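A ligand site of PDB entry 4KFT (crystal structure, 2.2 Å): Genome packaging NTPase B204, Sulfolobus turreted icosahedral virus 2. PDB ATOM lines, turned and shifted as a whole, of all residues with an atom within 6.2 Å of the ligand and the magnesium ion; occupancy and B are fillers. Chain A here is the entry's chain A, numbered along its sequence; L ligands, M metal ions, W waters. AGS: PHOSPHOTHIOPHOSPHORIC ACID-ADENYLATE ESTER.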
ATOM      1  N   GLY A  11     -16.946 -14.825  -1.903  1.00  0.00           N
ATOM      2  CA  GLY A  11     -18.346 -15.123  -2.156  1.00  0.00           C
ATOM      3  C   GLY A  11     -18.515 -16.434  -2.895  1.00  0.00           C
ATOM      4  O   GLY A  11     -17.689 -16.793  -3.746  1.00  0.00           O
ATOM      5  N   ARG A  12     -19.598 -17.137  -2.561  1.00  0.00           N
ATOM      6  CA  ARG A  12     -19.991 -18.382  -3.217  1.00  0.00           C
ATOM      7  C   ARG A  12     -20.004 -18.243  -4.747  1.00  0.00           C
ATOM      8  O   ARG A  12     -20.110 -17.132  -5.272  1.00  0.00           O
ATOM      9  CB  ARG A  12     -21.365 -18.822  -2.697  1.00  0.00           C
ATOM     10  N   LYS A  13     -19.858 -19.357  -5.456  1.00  0.00           N
ATOM     11  CA  LYS A  13     -19.857 -19.348  -6.915  1.00  0.00           C
ATOM     12  C   LYS A  13     -21.156 -18.735  -7.418  1.00  0.00           C
ATOM     13  O   LYS A  13     -22.219 -18.986  -6.835  1.00  0.00           O
ATOM     14  CB  LYS A  13     -19.707 -20.763  -7.449  1.00  0.00           C
ATOM     15  CG  LYS A  13     -19.901 -20.877  -8.940  1.00  0.00           C
ATOM     16  CD  LYS A  13     -19.669 -22.300  -9.418  1.00  0.00           C
ATOM     17  CE  LYS A  13     -19.978 -22.434 -10.916  1.00  0.00           C
ATOM     18  NZ  LYS A  13     -19.214 -21.432 -11.725  1.00  0.00           N
ATOM     19  N   LYS A  14     -21.047 -17.905  -8.453  1.00  0.00           N
ATOM     20  CA  LYS A  14     -22.156 -17.159  -9.054  1.00  0.00           C
ATOM     21  C   LYS A  14     -22.528 -15.891  -8.322  1.00  0.00           C
ATOM     22  O   LYS A  14     -23.462 -15.219  -8.734  1.00  0.00           O
ATOM     23  CB  LYS A  14     -23.402 -18.026  -9.294  1.00  0.00           C
ATOM     24  CG  LYS A  14     -23.191 -19.141 -10.301  1.00  0.00           C
ATOM     25  CD  LYS A  14     -24.179 -19.048 -11.453  1.00  0.00           C
ATOM     26  N   SER A  15     -21.816 -15.524  -7.261  1.00  0.00           N
ATOM     27  CA  SER A  15     -22.155 -14.275  -6.579  1.00  0.00           C
ATOM     28  C   SER A  15     -21.665 -13.000  -7.295  1.00  0.00           C
ATOM     29  O   SER A  15     -22.229 -11.923  -7.099  1.00  0.00           O
ATOM     30  CB  SER A  15     -21.809 -14.274  -5.078  1.00  0.00           C
ATOM     31  OG  SER A  15     -20.501 -14.686  -4.800  1.00  0.00           O
ATOM     32  N   GLY A  16     -20.656 -13.151  -8.155  1.00  0.00           N
ATOM     33  CA  GLY A  16     -20.220 -12.045  -8.991  1.00  0.00           C
ATOM     34  C   GLY A  16     -18.767 -11.633  -8.881  1.00  0.00           C
ATOM     35  O   GLY A  16     -18.405 -10.515  -9.255  1.00  0.00           O
ATOM     36  N   LYS A  17     -17.908 -12.534  -8.395  1.00  0.00           N
ATOM     37  CA  LYS A  17     -16.502 -12.196  -8.200  1.00  0.00           C
ATOM     38  C   LYS A  17     -15.787 -11.892  -9.513  1.00  0.00           C
ATOM     39  O   LYS A  17     -15.094 -10.882  -9.625  1.00  0.00           O
ATOM     40  CB  LYS A  17     -15.787 -13.304  -7.429  1.00  0.00           C
ATOM     41  CG  LYS A  17     -16.407 -13.566  -6.055  1.00  0.00           C
ATOM     42  CD  LYS A  17     -15.579 -14.563  -5.274  1.00  0.00           C
ATOM     43  CE  LYS A  17     -15.422 -15.845  -6.053  1.00  0.00           C
ATOM     44  NZ  LYS A  17     -16.717 -16.526  -6.289  1.00  0.00           N
ATOM     45  N   SER A  18     -15.971 -12.752 -10.511  1.00  0.00           N
ATOM     46  CA  SER A  18     -15.284 -12.567 -11.789  1.00  0.00           C
ATOM     47  C   SER A  18     -15.817 -11.351 -12.549  1.00  0.00           C
ATOM     48  O   SER A  18     -15.062 -10.622 -13.203  1.00  0.00           O
ATOM     49  CB  SER A  18     -15.340 -13.861 -12.616  1.00  0.00           C
ATOM     50  OG  SER A  18     -14.634 -14.912 -11.964  1.00  0.00           O
ATOM     51  N   TYR A  19     -17.124 -11.129 -12.432  1.00  0.00           N
ATOM     52  CA  TYR A  19     -17.744  -9.926 -12.982  1.00  0.00           C
ATOM     53  C   TYR A  19     -17.111  -8.634 -12.489  1.00  0.00           C
ATOM     54  O   TYR A  19     -16.814  -7.736 -13.272  1.00  0.00           O
ATOM     55  CB  TYR A  19     -19.239  -9.913 -12.656  1.00  0.00           C
ATOM     56  CG  TYR A  19     -20.062  -8.990 -13.517  1.00  0.00           C
ATOM     57  CD1 TYR A  19     -20.646  -9.452 -14.703  1.00  0.00           C
ATOM     58  CD2 TYR A  19     -20.296  -7.673 -13.146  1.00  0.00           C
ATOM     59  CE1 TYR A  19     -21.425  -8.606 -15.505  1.00  0.00           C
ATOM     60  CE2 TYR A  19     -21.065  -6.820 -13.936  1.00  0.00           C
ATOM     61  CZ  TYR A  19     -21.632  -7.291 -15.115  1.00  0.00           C
ATOM     62  OH  TYR A  19     -22.412  -6.455 -15.895  1.00  0.00           O
ATOM     63  N   LEU A  20     -16.914  -8.550 -11.171  1.00  0.00           N
ATOM     64  CA  LEU A  20     -16.226  -7.429 -10.524  1.00  0.00           C
ATOM     65  C   LEU A  20     -14.820  -7.234 -11.084  1.00  0.00           C
ATOM     66  O   LEU A  20     -14.372  -6.121 -11.316  1.00  0.00           O
ATOM     67  CB  LEU A  20     -16.126  -7.694  -9.020  1.00  0.00           C
ATOM     68  CG  LEU A  20     -16.315  -6.579  -8.007  1.00  0.00           C
ATOM     69  CD1 LEU A  20     -17.580  -5.862  -8.299  1.00  0.00           C
ATOM     70  CD2 LEU A  20     -16.355  -7.136  -6.593  1.00  0.00           C
ATOM     71  N   LYS A  22     -13.706  -8.341 -14.087  1.00  0.00           N
ATOM     72  CA  LYS A  22     -13.858  -8.000 -15.505  1.00  0.00           C
ATOM     73  C   LYS A  22     -14.415  -6.602 -15.704  1.00  0.00           C
ATOM     74  O   LYS A  22     -14.082  -5.934 -16.677  1.00  0.00           O
ATOM     75  CB  LYS A  22     -14.768  -9.018 -16.212  1.00  0.00           C
ATOM     76  CG  LYS A  22     -14.155 -10.382 -16.426  1.00  0.00           C
ATOM     77  CD  LYS A  22     -15.194 -11.380 -16.920  1.00  0.00           C
ATOM     78  CE  LYS A  22     -14.816 -12.823 -16.561  1.00  0.00           C
ATOM     79  NZ  LYS A  22     -16.019 -13.733 -16.443  1.00  0.00           N
ATOM     80  N   ASN A  42      -9.207 -22.035 -14.102  1.00  0.00           N
ATOM     81  CA  ASN A  42     -10.438 -22.647 -14.597  1.00  0.00           C
ATOM     82  C   ASN A  42     -10.735 -22.321 -16.063  1.00  0.00           C
ATOM     83  O   ASN A  42     -11.034 -23.214 -16.865  1.00  0.00           O
ATOM     84  CB  ASN A  42     -11.633 -22.227 -13.725  1.00  0.00           C
ATOM     85  CG  ASN A  42     -11.831 -20.716 -13.687  1.00  0.00           C
ATOM     86  OD1 ASN A  42     -12.284 -20.107 -14.669  1.00  0.00           O
ATOM     87  ND2 ASN A  42     -11.540 -20.111 -12.537  1.00  0.00           N
ATOM     88  N   GLU A  49     -12.130 -18.344 -19.564  1.00  0.00           N
ATOM     89  CA  GLU A  49     -13.002 -17.272 -19.062  1.00  0.00           C
ATOM     90  C   GLU A  49     -12.449 -15.852 -19.249  1.00  0.00           C
ATOM     91  O   GLU A  49     -13.200 -14.908 -19.492  1.00  0.00           O
ATOM     92  CB  GLU A  49     -13.334 -17.548 -17.593  1.00  0.00           C
ATOM     93  CG  GLU A  49     -13.917 -16.381 -16.817  1.00  0.00           C
ATOM     94  CD  GLU A  49     -14.521 -16.800 -15.482  1.00  0.00           C
ATOM     95  OE1 GLU A  49     -14.033 -17.758 -14.847  1.00  0.00           O
ATOM     96  OE2 GLU A  49     -15.523 -16.161 -15.072  1.00  0.00           O
ATOM     97  N   TYR A  50     -11.137 -15.694 -19.142  1.00  0.00           N
ATOM     98  CA  TYR A  50     -10.515 -14.387 -19.288  1.00  0.00           C
ATOM     99  C   TYR A  50      -9.761 -14.184 -20.624  1.00  0.00           C
ATOM    100  O   TYR A  50      -9.138 -13.152 -20.834  1.00  0.00           O
ATOM    101  CB  TYR A  50      -9.577 -14.113 -18.104  1.00  0.00           C
ATOM    102  CG  TYR A  50     -10.238 -14.048 -16.740  1.00  0.00           C
ATOM    103  CD1 TYR A  50     -10.733 -12.836 -16.232  1.00  0.00           C
ATOM    104  CD2 TYR A  50     -10.352 -15.179 -15.945  1.00  0.00           C
ATOM    105  CE1 TYR A  50     -11.321 -12.768 -14.964  1.00  0.00           C
ATOM    106  CE2 TYR A  50     -10.942 -15.122 -14.686  1.00  0.00           C
ATOM    107  CZ  TYR A  50     -11.429 -13.916 -14.206  1.00  0.00           C
ATOM    108  OH  TYR A  50     -12.017 -13.882 -12.953  1.00  0.00           O
ATOM    109  N   ASP A 103      -7.640 -15.895  -9.733  1.00  0.00           N
ATOM    110  CA  ASP A 103      -9.054 -16.225  -9.552  1.00  0.00           C
ATOM    111  C   ASP A 103      -9.298 -17.502  -8.734  1.00  0.00           C
ATOM    112  O   ASP A 103     -10.440 -17.931  -8.563  1.00  0.00           O
ATOM    113  CB  ASP A 103      -9.796 -16.304 -10.897  1.00  0.00           C
ATOM    114  CG  ASP A 103     -11.288 -15.972 -10.768  1.00  0.00           C
ATOM    115  OD1 ASP A 103     -11.659 -14.797 -10.978  1.00  0.00           O
ATOM    116  OD2 ASP A 103     -12.085 -16.885 -10.471  1.00  0.00           O
ATOM    117  N   SER A 136      -9.056 -14.302  -5.090  1.00  0.00           N
ATOM    118  CA  SER A 136     -10.473 -14.619  -5.197  1.00  0.00           C
ATOM    119  C   SER A 136     -10.753 -15.938  -4.498  1.00  0.00           C
ATOM    120  O   SER A 136      -9.999 -16.900  -4.663  1.00  0.00           O
ATOM    121  CB  SER A 136     -10.847 -14.729  -6.675  1.00  0.00           C
ATOM    122  OG  SER A 136     -12.235 -14.735  -6.844  1.00  0.00           O
ATOM    123  N   PHE A 157     -19.455 -10.753  -0.772  1.00  0.00           N
ATOM    124  CA  PHE A 157     -20.862 -10.905  -1.151  1.00  0.00           C
ATOM    125  C   PHE A 157     -21.633 -11.607  -0.042  1.00  0.00           C
ATOM    126  O   PHE A 157     -21.040 -12.087   0.935  1.00  0.00           O
ATOM    127  CB  PHE A 157     -21.000 -11.689  -2.477  1.00  0.00           C
ATOM    128  CG  PHE A 157     -20.362 -10.986  -3.645  1.00  0.00           C
ATOM    129  CD1 PHE A 157     -21.120 -10.210  -4.502  1.00  0.00           C
ATOM    130  CD2 PHE A 157     -18.990 -11.089  -3.862  1.00  0.00           C
ATOM    131  CE1 PHE A 157     -20.525  -9.549  -5.579  1.00  0.00           C
ATOM    132  CE2 PHE A 157     -18.394 -10.439  -4.926  1.00  0.00           C
ATOM    133  CZ  PHE A 157     -19.161  -9.658  -5.786  1.00  0.00           C
ATOM    134  N   GLN A 185     -28.628  -9.569  -4.247  1.00  0.00           N
ATOM    135  CA  GLN A 185     -27.819 -10.132  -5.328  1.00  0.00           C
ATOM    136  C   GLN A 185     -26.900  -9.093  -5.962  1.00  0.00           C
ATOM    137  O   GLN A 185     -27.325  -7.973  -6.263  1.00  0.00           O
ATOM    138  CB  GLN A 185     -28.704 -10.770  -6.396  1.00  0.00           C
ATOM    139  CG  GLN A 185     -27.922 -11.544  -7.444  1.00  0.00           C
ATOM    140  CD  GLN A 185     -28.820 -12.339  -8.381  1.00  0.00           C
ATOM    141  OE1 GLN A 185     -29.762 -11.805  -8.959  1.00  0.00           O
ATOM    142  NE2 GLN A 185     -28.547 -13.634  -8.513  1.00  0.00           N
ATOM    143  N   TYR A 186     -25.628  -9.468  -6.103  1.00  0.00           N
ATOM    144  CA  TYR A 186     -24.584  -8.654  -6.745  1.00  0.00           C
ATOM    145  C   TYR A 186     -24.208  -7.418  -5.964  1.00  0.00           C
ATOM    146  O   TYR A 186     -23.334  -6.664  -6.399  1.00  0.00           O
ATOM    147  CB  TYR A 186     -24.959  -8.252  -8.183  1.00  0.00           C
ATOM    148  CG  TYR A 186     -25.427  -9.397  -9.038  1.00  0.00           C
ATOM    149  CD1 TYR A 186     -24.798 -10.634  -8.965  1.00  0.00           C
ATOM    150  CD2 TYR A 186     -26.506  -9.244  -9.899  1.00  0.00           C
ATOM    151  CE1 TYR A 186     -25.228 -11.694  -9.741  1.00  0.00           C
ATOM    152  CE2 TYR A 186     -26.947 -10.298 -10.669  1.00  0.00           C
ATOM    153  CZ  TYR A 186     -26.309 -11.517 -10.596  1.00  0.00           C
ATOM    154  OH  TYR A 186     -26.758 -12.566 -11.369  1.00  0.00           O
ATOM    155  N   PRO A 203     -24.751  -3.086  -7.096  1.00  0.00           N
ATOM    156  CA  PRO A 203     -24.152  -3.855  -8.186  1.00  0.00           C
ATOM    157  C   PRO A 203     -23.446  -2.978  -9.199  1.00  0.00           C
ATOM    158  O   PRO A 203     -23.910  -1.872  -9.508  1.00  0.00           O
ATOM    159  CB  PRO A 203     -25.359  -4.510  -8.867  1.00  0.00           C
ATOM    160  CG  PRO A 203     -26.360  -4.627  -7.796  1.00  0.00           C
ATOM    161  CD  PRO A 203     -26.163  -3.438  -6.889  1.00  0.00           C
ATOM    162  N   ILE A 204     -22.325  -3.480  -9.707  1.00  0.00           N
ATOM    163  CA  ILE A 204     -21.649  -2.876 -10.855  1.00  0.00           C
ATOM    164  C   ILE A 204     -22.552  -2.855 -12.107  1.00  0.00           C
ATOM    165  O   ILE A 204     -23.293  -3.808 -12.357  1.00  0.00           O
ATOM    166  CB  ILE A 204     -20.347  -3.658 -11.154  1.00  0.00           C
ATOM    167  CG1 ILE A 204     -19.365  -3.476  -9.992  1.00  0.00           C
ATOM    168  CG2 ILE A 204     -19.723  -3.261 -12.479  1.00  0.00           C
ATOM    169  CD1 ILE A 204     -19.296  -2.053  -9.461  1.00  0.00           C
ATOM    170  N   LEU A 205     -22.498  -1.781 -12.886  1.00  0.00           N
ATOM    171  CA  LEU A 205     -23.180  -1.754 -14.182  1.00  0.00           C
ATOM    172  C   LEU A 205     -22.323  -2.234 -15.370  1.00  0.00           C
ATOM    173  O   LEU A 205     -21.360  -1.582 -15.771  1.00  0.00           O
ATOM    174  CB  LEU A 205     -23.762  -0.369 -14.460  1.00  0.00           C
ATOM    175  CG  LEU A 205     -25.168  -0.222 -13.871  1.00  0.00           C
ATOM    176  CD1 LEU A 205     -25.646   1.219 -13.908  1.00  0.00           C
ATOM    177  CD2 LEU A 205     -26.158  -1.130 -14.590  1.00  0.00           C
HETATM  178  PB  AGS L   1     -18.482 -15.758  -9.667  1.00  0.00           P
HETATM  179  O1B AGS L   1     -18.465 -15.121  -8.252  1.00  0.00           O
HETATM  180  O2B AGS L   1     -18.762 -17.270  -9.545  1.00  0.00           O
HETATM  181  O3B AGS L   1     -17.114 -15.559 -10.344  1.00  0.00           O
HETATM  182  PA  AGS L   1     -19.646 -14.482 -11.906  1.00  0.00           P
HETATM  183  O1A AGS L   1     -18.687 -13.261 -11.993  1.00  0.00           O
HETATM  184  O2A AGS L   1     -19.249 -15.517 -12.981  1.00  0.00           O
HETATM  185  O3A AGS L   1     -19.677 -15.122 -10.473  1.00  0.00           O
HETATM  186  O5' AGS L   1     -21.068 -13.967 -12.246  1.00  0.00           O
HETATM  187  C5' AGS L   1     -22.163 -14.816 -12.298  1.00  0.00           C
HETATM  188  C4' AGS L   1     -23.333 -14.397 -13.119  1.00  0.00           C
HETATM  189  O4' AGS L   1     -24.006 -13.305 -12.586  1.00  0.00           O
HETATM  190  C3' AGS L   1     -22.928 -13.988 -14.508  1.00  0.00           C
HETATM  191  O3' AGS L   1     -23.939 -14.336 -15.382  1.00  0.00           O
HETATM  192  C2' AGS L   1     -22.832 -12.586 -14.451  1.00  0.00           C
HETATM  193  O2' AGS L   1     -23.156 -12.079 -15.694  1.00  0.00           O
HETATM  194  C1' AGS L   1     -23.842 -12.180 -13.429  1.00  0.00           C
HETATM  195  N9  AGS L   1     -23.430 -11.054 -12.671  1.00  0.00           N
HETATM  196  C8  AGS L   1     -22.519 -10.888 -11.717  1.00  0.00           C
HETATM  197  N7  AGS L   1     -22.551  -9.588 -11.370  1.00  0.00           N
HETATM  198  C5  AGS L   1     -23.483  -8.942 -12.104  1.00  0.00           C
HETATM  199  C6  AGS L   1     -23.919  -7.625 -12.138  1.00  0.00           C
HETATM  200  N6  AGS L   1     -23.388  -6.604 -11.305  1.00  0.00           N
HETATM  201  N1  AGS L   1     -24.890  -7.303 -13.022  1.00  0.00           N
HETATM  202  C2  AGS L   1     -25.427  -8.228 -13.832  1.00  0.00           C
HETATM  203  N3  AGS L   1     -25.003  -9.493 -13.790  1.00  0.00           N
HETATM  204  C4  AGS L   1     -24.046  -9.888 -12.938  1.00  0.00           C
HETATM  205 MG    MG M   1     -15.541 -16.605 -11.371  1.00  0.00          MG
HETATM  206  O   HOH W   1     -19.979 -18.482 -11.833  1.00  0.00           O
HETATM  207  O   HOH W   2     -16.972 -16.655 -12.927  1.00  0.00           O
HETATM  208  O   HOH W   3     -18.113 -13.160 -14.903  1.00  0.00           O
HETATM  209  O   HOH W   4     -19.493 -16.738 -15.343  1.00  0.00           O
HETATM  210  O   HOH W   5     -25.705 -15.297 -10.439  1.00  0.00           O
HETATM  211  O   HOH W   6     -20.396  -8.698  -9.801  1.00  0.00           O
HETATM  212  O   HOH W   7     -21.566  -6.246  -8.737  1.00  0.00           O
HETATM  213  O   HOH W   8     -14.401 -16.505  -9.611  1.00  0.00           O
HETATM  214  O   HOH W   9     -14.148 -17.758 -12.386  1.00  0.00           O
HETATM  215  O   HOH W  10     -25.598 -11.047 -17.212  1.00  0.00           O
HETATM  216  O   HOH W  11     -16.664 -18.188 -10.627  1.00  0.00           O
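NZ of Lys 17 is in hydrogen-bond range of O of Gly 11, 2.7 Å away.
The side-chain hydroxyl (OG) of Ser 15 lies within hydrogen-bond range of the backbone carbonyl oxygen (O) of Arg 12, 2.5 Å away.
The side-chain carboxylate (OD1) of Asp 103 lies close to the side-chain hydroxyl (OG) of Ser 18 (3.1 Å).
OG of Ser 18 sits close to OE2 of Glu 49 (3.5 Å).
OG of Ser 18 lies close to OH of Tyr 50 (3.0 Å).
The side-chain carboxylate (OE2) of Glu 49 is in salt-bridge range of the side-chain amino group (NZ) of Lys 22 (2.8 Å).
The side-chain carboxylate (OE1) of Glu 49 lies close to the side-chain amide oxygen (OD1) of Asn 42, 2.9 Å away.
Residues that only touch the magnesium ion: Asp 103 (3.6 Å) and Glu 49 (3.7 Å).
Within 4 Å of the magnesium ion: Ser 18, Glu 49 and Asp 103.
The nearest printed residue that does not touch the magnesium ion is Tyr 50 (4.7 Å).
Water W2 lies within hydrogen-bond range of O2A of the ligand (2.5 Å) and OE2 of Glu 49 (2.6 Å).
Water W6 lies within hydrogen-bond range of O of Gly 16 and N7 of the ligand.
Water W1 bridges O2B of the ligand (2.9 Å) and NZ of Lys 13 (3.0 Å).
Water W3 lies within hydrogen-bond range of NZ of Lys 22 (2.7 Å), O1A of the ligand (3.0 Å) and N of Tyr 19 (3.3 Å).
Water W7 lies within hydrogen-bond range of O of Tyr 186 (3.0 Å), N of Ile 204 (3.0 Å) and N6 of the ligand (3.2 Å).
Water W5 lies within hydrogen-bond range of O of Lys 14 (2.8 Å), OH of Tyr 186 (3.1 Å) and O4' of the ligand (3.4 Å).
The backbone NH (N) of Lys 17 sits at hydrogen-bond distance from an oxygen (O1B) of the ligand, at 2.7 Å.
O1B of the ligand is in hydrogen-bond range of N of Gly 16, 2.9 Å away.
The backbone carbonyl oxygen (O) of Ile 204 lies within hydrogen-bond range of a nitrogen (N6) of the ligand (3.0 Å).
The side-chain hydroxyl (OH) of Tyr 186 is in hydrogen-bond range of an oxygen (O4') of the ligand (3.1 Å).
O1B of the ligand is in salt-bridge range of NZ of Lys 17 (3.0 Å).
The backbone NH of Lys 14 is in hydrogen-bond range of an oxygen (O2B) of the ligand (2.6 Å).
The backbone NH of Ser 18 lies within hydrogen-bond range of an oxygen (O1A) of the ligand (3.1 Å).
The backbone NH of Tyr 19 is in hydrogen-bond range of an oxygen (O1A) of the ligand, at 2.7 Å.
Arg 12 touches the ligand (O to O1B, 3.95 Å).
Lys 13 touches the ligand (C to O2B, 3.5 Å).
Ser 15 touches the ligand.
Pro 203 touches the ligand.
Hydrophobic or aromatic side chains within 4 Å of the ligand: Tyr 19, Tyr 186 and Pro 203.
Within 4 Å of the ligand: Arg 12, Lys 13, Lys 14, Ser 15, Gly 16, Lys 17, Ser 18, Tyr 19, Tyr 186, Pro 203 and Ile 204.
The nearest printed residue that does not touch the ligand is Glu 49 (4.3 Å).
The side-chain hydroxyl (OG) of Ser 18 binds the magnesium ion, 2.0 Å away.
The magnesium ion is bound by water W9, 2.1 Å away.
Water W11 binds the magnesium ion (2.1 Å).
The magnesium ion is bound by water W8, 2.1 Å away.
The magnesium ion is bound by water W2.
The magnesium ion is bound by O3B of the ligand, at 2.2 Å.
The magnesium ion has six donor atoms within binding distance.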
